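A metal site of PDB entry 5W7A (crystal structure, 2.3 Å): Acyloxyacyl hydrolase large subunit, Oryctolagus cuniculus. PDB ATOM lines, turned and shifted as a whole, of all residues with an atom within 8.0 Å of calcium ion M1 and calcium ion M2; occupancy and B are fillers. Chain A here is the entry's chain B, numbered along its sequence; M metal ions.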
ATOM      1  N   PRO A  27       6.802  -1.746  -2.182  1.00  0.00           N
ATOM      2  CA  PRO A  27       8.084  -2.149  -2.764  1.00  0.00           C
ATOM      3  C   PRO A  27       7.890  -2.880  -4.087  1.00  0.00           C
ATOM      4  O   PRO A  27       6.915  -3.597  -4.297  1.00  0.00           O
ATOM      5  CB  PRO A  27       8.690  -3.068  -1.704  1.00  0.00           C
ATOM      6  CG  PRO A  27       7.519  -3.585  -0.937  1.00  0.00           C
ATOM      7  CD  PRO A  27       6.531  -2.456  -0.912  1.00  0.00           C
ATOM      8  N   LYS A  29      10.422  -4.964  -5.179  1.00  0.00           N
ATOM      9  CA  LYS A  29      10.985  -6.266  -4.823  1.00  0.00           C
ATOM     10  C   LYS A  29      10.245  -6.794  -3.605  1.00  0.00           C
ATOM     11  O   LYS A  29      10.464  -6.342  -2.473  1.00  0.00           O
ATOM     12  CB  LYS A  29      12.484  -6.119  -4.573  1.00  0.00           C
ATOM     13  CG  LYS A  29      13.241  -7.379  -4.182  1.00  0.00           C
ATOM     14  CD  LYS A  29      12.940  -8.554  -5.085  1.00  0.00           C
ATOM     15  CE  LYS A  29      14.089  -9.545  -5.060  1.00  0.00           C
ATOM     16  NZ  LYS A  29      13.750 -10.803  -5.756  1.00  0.00           N
ATOM     17  N   ASP A  30       9.342  -7.756  -3.829  1.00  0.00           N
ATOM     18  CA  ASP A  30       8.451  -8.264  -2.789  1.00  0.00           C
ATOM     19  C   ASP A  30       7.717  -9.495  -3.299  1.00  0.00           C
ATOM     20  O   ASP A  30       6.564  -9.398  -3.735  1.00  0.00           O
ATOM     21  CB  ASP A  30       7.442  -7.177  -2.390  1.00  0.00           C
ATOM     22  CG  ASP A  30       6.510  -7.633  -1.287  1.00  0.00           C
ATOM     23  OD1 ASP A  30       6.823  -8.631  -0.607  1.00  0.00           O
ATOM     24  OD2 ASP A  30       5.463  -6.983  -1.106  1.00  0.00           O
ATOM     25  N   VAL A  31       8.363 -10.660  -3.271  1.00  0.00           N
ATOM     26  CA  VAL A  31       7.817 -11.805  -3.978  1.00  0.00           C
ATOM     27  C   VAL A  31       6.492 -12.236  -3.362  1.00  0.00           C
ATOM     28  O   VAL A  31       5.522 -12.513  -4.076  1.00  0.00           O
ATOM     29  CB  VAL A  31       8.825 -12.962  -4.017  1.00  0.00           C
ATOM     30  CG1 VAL A  31       8.245 -14.153  -4.783  1.00  0.00           C
ATOM     31  CG2 VAL A  31      10.117 -12.500  -4.670  1.00  0.00           C
ATOM     32  N   ASP A  32       6.413 -12.294  -2.030  1.00  0.00           N
ATOM     33  CA  ASP A  32       5.190 -12.742  -1.375  1.00  0.00           C
ATOM     34  C   ASP A  32       4.157 -11.629  -1.236  1.00  0.00           C
ATOM     35  O   ASP A  32       3.078 -11.874  -0.687  1.00  0.00           O
ATOM     36  CB  ASP A  32       5.512 -13.320   0.009  1.00  0.00           C
ATOM     37  CG  ASP A  32       6.265 -12.349   0.900  1.00  0.00           C
ATOM     38  OD1 ASP A  32       6.159 -11.138   0.665  1.00  0.00           O
ATOM     39  OD2 ASP A  32       6.944 -12.815   1.834  1.00  0.00           O
ATOM     40  N   SER A  33       4.450 -10.428  -1.718  1.00  0.00           N
ATOM     41  CA  SER A  33       3.463  -9.336  -1.756  1.00  0.00           C
ATOM     42  C   SER A  33       2.874  -9.041  -0.386  1.00  0.00           C
ATOM     43  O   SER A  33       1.660  -8.843  -0.251  1.00  0.00           O
ATOM     44  CB  SER A  33       2.354  -9.651  -2.762  1.00  0.00           C
ATOM     45  OG  SER A  33       2.875  -9.791  -4.072  1.00  0.00           O
ATOM     46  N   ASP A  34       3.715  -9.004   0.650  1.00  0.00           N
ATOM     47  CA  ASP A  34       3.249  -8.588   1.975  1.00  0.00           C
ATOM     48  C   ASP A  34       3.678  -7.166   2.310  1.00  0.00           C
ATOM     49  O   ASP A  34       3.415  -6.705   3.428  1.00  0.00           O
ATOM     50  CB  ASP A  34       3.746  -9.570   3.052  1.00  0.00           C
ATOM     51  CG  ASP A  34       5.263  -9.640   3.145  1.00  0.00           C
ATOM     52  OD1 ASP A  34       5.948  -8.721   2.638  1.00  0.00           O
ATOM     53  OD2 ASP A  34       5.753 -10.614   3.739  1.00  0.00           O
ATOM     54  N   LYS A  35       4.320  -6.465   1.382  1.00  0.00           N
ATOM     55  CA  LYS A  35       4.725  -5.050   1.432  1.00  0.00           C
ATOM     56  C   LYS A  35       6.058  -4.867   2.130  1.00  0.00           C
ATOM     57  O   LYS A  35       6.502  -3.726   2.304  1.00  0.00           O
ATOM     58  CB  LYS A  35       3.677  -4.135   2.105  1.00  0.00           C
ATOM     59  CG  LYS A  35       2.549  -3.802   1.169  1.00  0.00           C
ATOM     60  CD  LYS A  35       1.251  -3.566   1.896  1.00  0.00           C
ATOM     61  CE  LYS A  35       0.158  -3.196   0.920  1.00  0.00           C
ATOM     62  NZ  LYS A  35      -1.168  -3.381   1.535  1.00  0.00           N
ATOM     63  N   TYR A  36       6.718  -5.944   2.532  1.00  0.00           N
ATOM     64  CA  TYR A  36       8.045  -5.870   3.132  1.00  0.00           C
ATOM     65  C   TYR A  36       9.049  -6.510   2.193  1.00  0.00           C
ATOM     66  O   TYR A  36       8.750  -7.516   1.540  1.00  0.00           O
ATOM     67  CB  TYR A  36       8.048  -6.573   4.495  1.00  0.00           C
ATOM     68  CG  TYR A  36       7.165  -5.876   5.502  1.00  0.00           C
ATOM     69  CD1 TYR A  36       7.654  -4.823   6.273  1.00  0.00           C
ATOM     70  CD2 TYR A  36       5.841  -6.246   5.685  1.00  0.00           C
ATOM     71  CE1 TYR A  36       6.850  -4.184   7.198  1.00  0.00           C
ATOM     72  CE2 TYR A  36       5.028  -5.604   6.607  1.00  0.00           C
ATOM     73  CZ  TYR A  36       5.540  -4.575   7.354  1.00  0.00           C
ATOM     74  OH  TYR A  36       4.749  -3.935   8.273  1.00  0.00           O
ATOM     75  N   SER A  37      10.232  -5.920   2.112  1.00  0.00           N
ATOM     76  CA  SER A  37      11.184  -6.236   1.063  1.00  0.00           C
ATOM     77  C   SER A  37      12.502  -6.704   1.661  1.00  0.00           C
ATOM     78  O   SER A  37      12.788  -6.464   2.851  1.00  0.00           O
ATOM     79  CB  SER A  37      11.410  -5.017   0.157  1.00  0.00           C
ATOM     80  OG  SER A  37      12.309  -5.292  -0.898  1.00  0.00           O
ATOM     81  N   ILE A  38      13.300  -7.393   0.843  1.00  0.00           N
ATOM     82  CA  ILE A  38      14.702  -7.637   1.139  1.00  0.00           C
ATOM     83  C   ILE A  38      15.619  -6.676   0.401  1.00  0.00           C
ATOM     84  O   ILE A  38      16.846  -6.776   0.527  1.00  0.00           O
ATOM     85  CB  ILE A  38      15.102  -9.098   0.834  1.00  0.00           C
ATOM     86  CG1 ILE A  38      14.967  -9.381  -0.671  1.00  0.00           C
ATOM     87  CG2 ILE A  38      14.234 -10.059   1.653  1.00  0.00           C
ATOM     88  CD1 ILE A  38      15.355 -10.787  -1.089  1.00  0.00           C
ATOM     89  N   GLY A  49      10.399  -2.274   7.948  1.00  0.00           N
ATOM     90  CA  GLY A  49      11.216  -3.383   8.408  1.00  0.00           C
ATOM     91  C   GLY A  49      11.508  -4.397   7.325  1.00  0.00           C
ATOM     92  O   GLY A  49      10.641  -4.720   6.497  1.00  0.00           O
ATOM     93  N   ARG A  50      12.727  -4.912   7.316  1.00  0.00           N
ATOM     94  CA  ARG A  50      13.129  -5.899   6.318  1.00  0.00           C
ATOM     95  C   ARG A  50      12.379  -7.221   6.516  1.00  0.00           C
ATOM     96  O   ARG A  50      12.275  -7.724   7.645  1.00  0.00           O
ATOM     97  CB  ARG A  50      14.631  -6.136   6.392  1.00  0.00           C
ATOM     98  CG  ARG A  50      15.182  -6.842   5.170  1.00  0.00           C
ATOM     99  CD  ARG A  50      16.474  -7.589   5.471  1.00  0.00           C
ATOM    100  NE  ARG A  50      17.563  -6.704   5.888  1.00  0.00           N
ATOM    101  CZ  ARG A  50      18.592  -6.335   5.134  1.00  0.00           C
ATOM    102  NH1 ARG A  50      18.704  -6.761   3.880  1.00  0.00           N
ATOM    103  NH2 ARG A  50      19.527  -5.525   5.625  1.00  0.00           N
ATOM    104  N   ASP A  51      11.892  -7.784   5.415  1.00  0.00           N
ATOM    105  CA  ASP A  51      11.188  -9.061   5.418  1.00  0.00           C
ATOM    106  C   ASP A  51      12.178 -10.196   5.639  1.00  0.00           C
ATOM    107  O   ASP A  51      13.010 -10.487   4.771  1.00  0.00           O
ATOM    108  CB  ASP A  51      10.455  -9.237   4.088  1.00  0.00           C
ATOM    109  CG  ASP A  51       9.452 -10.367   4.124  1.00  0.00           C
ATOM    110  OD1 ASP A  51       9.450 -11.142   5.099  1.00  0.00           O
ATOM    111  OD2 ASP A  51       8.664 -10.479   3.163  1.00  0.00           O
ATOM    112  N   CYS A  52      12.090 -10.866   6.785  1.00  0.00           N
ATOM    113  CA  CYS A  52      12.987 -11.986   7.065  1.00  0.00           C
ATOM    114  C   CYS A  52      12.605 -13.252   6.298  1.00  0.00           C
ATOM    115  O   CYS A  52      13.382 -14.215   6.319  1.00  0.00           O
ATOM    116  CB  CYS A  52      13.026 -12.274   8.575  1.00  0.00           C
ATOM    117  SG  CYS A  52      11.435 -12.636   9.383  1.00  0.00           S
ATOM    118  N   ASN A  53      11.461 -13.281   5.612  1.00  0.00           N
ATOM    119  CA  ASN A  53      11.125 -14.355   4.666  1.00  0.00           C
ATOM    120  C   ASN A  53      10.226 -13.763   3.580  1.00  0.00           C
ATOM    121  O   ASN A  53       9.002 -13.696   3.736  1.00  0.00           O
ATOM    122  CB  ASN A  53      10.431 -15.527   5.356  1.00  0.00           C
ATOM    123  CG  ASN A  53      10.322 -16.756   4.457  1.00  0.00           C
ATOM    124  OD1 ASN A  53      10.263 -16.626   3.236  1.00  0.00           O
ATOM    125  ND2 ASN A  53      10.284 -17.950   5.059  1.00  0.00           N
ATOM    126  N   ASP A  54      10.837 -13.330   2.474  1.00  0.00           N
ATOM    127  CA  ASP A  54      10.064 -12.775   1.371  1.00  0.00           C
ATOM    128  C   ASP A  54       9.421 -13.844   0.500  1.00  0.00           C
ATOM    129  O   ASP A  54       8.951 -13.533  -0.595  1.00  0.00           O
ATOM    130  CB  ASP A  54      10.948 -11.860   0.503  1.00  0.00           C
ATOM    131  CG  ASP A  54      10.125 -10.997  -0.443  1.00  0.00           C
ATOM    132  OD1 ASP A  54       8.981 -10.656  -0.085  1.00  0.00           O
ATOM    133  OD2 ASP A  54      10.630 -10.653  -1.528  1.00  0.00           O
ATOM    134  N   SER A  55       9.393 -15.104   0.959  1.00  0.00           N
ATOM    135  CA  SER A  55       8.666 -16.175   0.297  1.00  0.00           C
ATOM    136  C   SER A  55       7.405 -16.571   1.039  1.00  0.00           C
ATOM    137  O   SER A  55       6.711 -17.489   0.587  1.00  0.00           O
ATOM    138  CB  SER A  55       9.568 -17.405   0.130  1.00  0.00           C
ATOM    139  OG  SER A  55      10.283 -17.360  -1.095  1.00  0.00           O
ATOM    140  N   ASP A  56       7.088 -15.930   2.163  1.00  0.00           N
ATOM    141  CA  ASP A  56       5.952 -16.322   2.987  1.00  0.00           C
ATOM    142  C   ASP A  56       5.188 -15.068   3.404  1.00  0.00           C
ATOM    143  O   ASP A  56       5.709 -14.226   4.145  1.00  0.00           O
ATOM    144  CB  ASP A  56       6.415 -17.107   4.217  1.00  0.00           C
ATOM    145  CG  ASP A  56       5.271 -17.802   4.931  1.00  0.00           C
ATOM    146  OD1 ASP A  56       4.121 -17.337   4.797  1.00  0.00           O
ATOM    147  OD2 ASP A  56       5.535 -18.810   5.620  1.00  0.00           O
ATOM    148  N   LYS A  57       3.951 -14.967   2.932  1.00  0.00           N
ATOM    149  CA  LYS A  57       3.091 -13.827   3.256  1.00  0.00           C
ATOM    150  C   LYS A  57       2.731 -13.762   4.737  1.00  0.00           C
ATOM    151  O   LYS A  57       2.318 -12.705   5.217  1.00  0.00           O
ATOM    152  CB  LYS A  57       1.827 -13.926   2.391  1.00  0.00           C
ATOM    153  CG  LYS A  57       0.923 -12.712   2.360  1.00  0.00           C
ATOM    154  CD  LYS A  57      -0.221 -12.939   1.365  1.00  0.00           C
ATOM    155  CE  LYS A  57      -1.434 -12.063   1.662  1.00  0.00           C
ATOM    156  NZ  LYS A  57      -1.291 -10.661   1.163  1.00  0.00           N
ATOM    157  N   THR A  58       2.887 -14.863   5.478  1.00  0.00           N
ATOM    158  CA  THR A  58       2.574 -14.898   6.903  1.00  0.00           C
ATOM    159  C   THR A  58       3.790 -14.633   7.782  1.00  0.00           C
ATOM    160  O   THR A  58       3.723 -14.837   8.997  1.00  0.00           O
ATOM    161  CB  THR A  58       1.968 -16.257   7.292  1.00  0.00           C
ATOM    162  OG1 THR A  58       2.943 -17.285   7.127  1.00  0.00           O
ATOM    163  CG2 THR A  58       0.756 -16.573   6.427  1.00  0.00           C
ATOM    164  N   VAL A  59       4.893 -14.182   7.192  1.00  0.00           N
ATOM    165  CA  VAL A  59       6.096 -13.808   7.936  1.00  0.00           C
ATOM    166  C   VAL A  59       6.409 -12.373   7.540  1.00  0.00           C
ATOM    167  O   VAL A  59       6.719 -12.093   6.374  1.00  0.00           O
ATOM    168  CB  VAL A  59       7.278 -14.741   7.623  1.00  0.00           C
ATOM    169  CG1 VAL A  59       8.539 -14.280   8.360  1.00  0.00           C
ATOM    170  CG2 VAL A  59       6.954 -16.165   7.995  1.00  0.00           C
ATOM    171  N   TYR A  60       6.316 -11.465   8.502  1.00  0.00           N
ATOM    172  CA  TYR A  60       6.546 -10.050   8.237  1.00  0.00           C
ATOM    173  C   TYR A  60       6.620  -9.330   9.584  1.00  0.00           C
ATOM    174  O   TYR A  60       6.107  -9.820  10.580  1.00  0.00           O
ATOM    175  CB  TYR A  60       5.431  -9.444   7.377  1.00  0.00           C
ATOM    176  CG  TYR A  60       4.051  -9.671   7.927  1.00  0.00           C
ATOM    177  CD1 TYR A  60       3.532  -8.837   8.899  1.00  0.00           C
ATOM    178  CD2 TYR A  60       3.279 -10.744   7.490  1.00  0.00           C
ATOM    179  CE1 TYR A  60       2.263  -9.051   9.421  1.00  0.00           C
ATOM    180  CE2 TYR A  60       2.014 -10.954   8.004  1.00  0.00           C
ATOM    181  CZ  TYR A  60       1.512 -10.107   8.967  1.00  0.00           C
ATOM    182  OH  TYR A  60       0.255 -10.329   9.480  1.00  0.00           O
ATOM    183  N   PRO A  61       7.233  -8.140   9.621  1.00  0.00           N
ATOM    184  CA  PRO A  61       7.344  -7.420  10.890  1.00  0.00           C
ATOM    185  C   PRO A  61       5.982  -6.963  11.400  1.00  0.00           C
ATOM    186  O   PRO A  61       5.083  -6.612  10.635  1.00  0.00           O
ATOM    187  CB  PRO A  61       8.231  -6.221  10.547  1.00  0.00           C
ATOM    188  CG  PRO A  61       8.891  -6.568   9.247  1.00  0.00           C
ATOM    189  CD  PRO A  61       7.895  -7.416   8.523  1.00  0.00           C
ATOM    190  N   SER A  74       8.379 -15.511  12.878  1.00  0.00           N
ATOM    191  CA  SER A  74       7.297 -15.131  11.972  1.00  0.00           C
ATOM    192  C   SER A  74       7.003 -13.632  11.965  1.00  0.00           C
ATOM    193  O   SER A  74       6.317 -13.165  11.051  1.00  0.00           O
ATOM    194  CB  SER A  74       6.017 -15.882  12.340  1.00  0.00           C
ATOM    195  OG  SER A  74       5.496 -15.419  13.577  1.00  0.00           O
ATOM    196  N   CYS A  76       9.695 -11.370  12.500  1.00  0.00           N
ATOM    197  CA  CYS A  76      10.950 -10.769  12.055  1.00  0.00           C
ATOM    198  C   CYS A  76      11.630  -9.896  13.118  1.00  0.00           C
ATOM    199  O   CYS A  76      12.481  -9.066  12.789  1.00  0.00           O
ATOM    200  CB  CYS A  76      10.745  -9.949  10.769  1.00  0.00           C
ATOM    201  SG  CYS A  76      10.333 -10.909   9.272  1.00  0.00           S
HETATM  202 CA    CA M   1       7.694  -9.482   1.287  1.00  0.00          CA
HETATM  203 CA    CA M   2       7.249 -12.255   4.102  1.00  0.00          CA
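OD2 of Asp 32 sits close to N of Ser 55 (3.5 Å). N of Asp 51 lies within hydrogen-bond range of O of Ser 37, at 3.0 Å. The side-chain sulfur (SG) of Cys 52 is disulfide-bonded to the side-chain sulfur (SG) of Cys 76 (2.1 Å). The side-chain carboxylate (OD1) of Asp 30 lies close to the backbone NH (N) of Ser 33 (3.2 Å). OD1 of Asn 53 lies within hydrogen-bond range of N of Ser 55 (2.9 Å). OD1 of Asp 56 sits at hydrogen-bond distance from OG1 of Thr 58 (2.6 Å). The backbone NH of Asp 56 is in hydrogen-bond range of the side-chain amide oxygen of Asn 53. The side-chain carboxylate (OD2) of Asp 30 sits at hydrogen-bond distance from the backbone NH (N) of Lys 35.
Calcium ion M1 is bound by the side-chain carboxylate of Asp 54 (2.2 Å), the backbone carbonyl oxygen of Tyr 36 (2.2 Å), the side-chain carboxylate of Asp 30 (2.3 Å), the side-chain carboxylate of Asp 34 (2.3 Å), the side-chain carboxylate of Asp 51 (2.3 Å) and the side-chain carboxylate of Asp 32 (2.3 Å).
Calcium ion M2 is bound by OD2 of Asp 34 (2.3 Å), O of Asn 53 (2.3 Å), O of Val 59 (2.3 Å), OD2 of Asp 32 (2.4 Å), OD2 of Asp 51 (2.5 Å), O of Asp 56 (2.5 Å) and OD1 of Asp 51 (2.7 Å).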
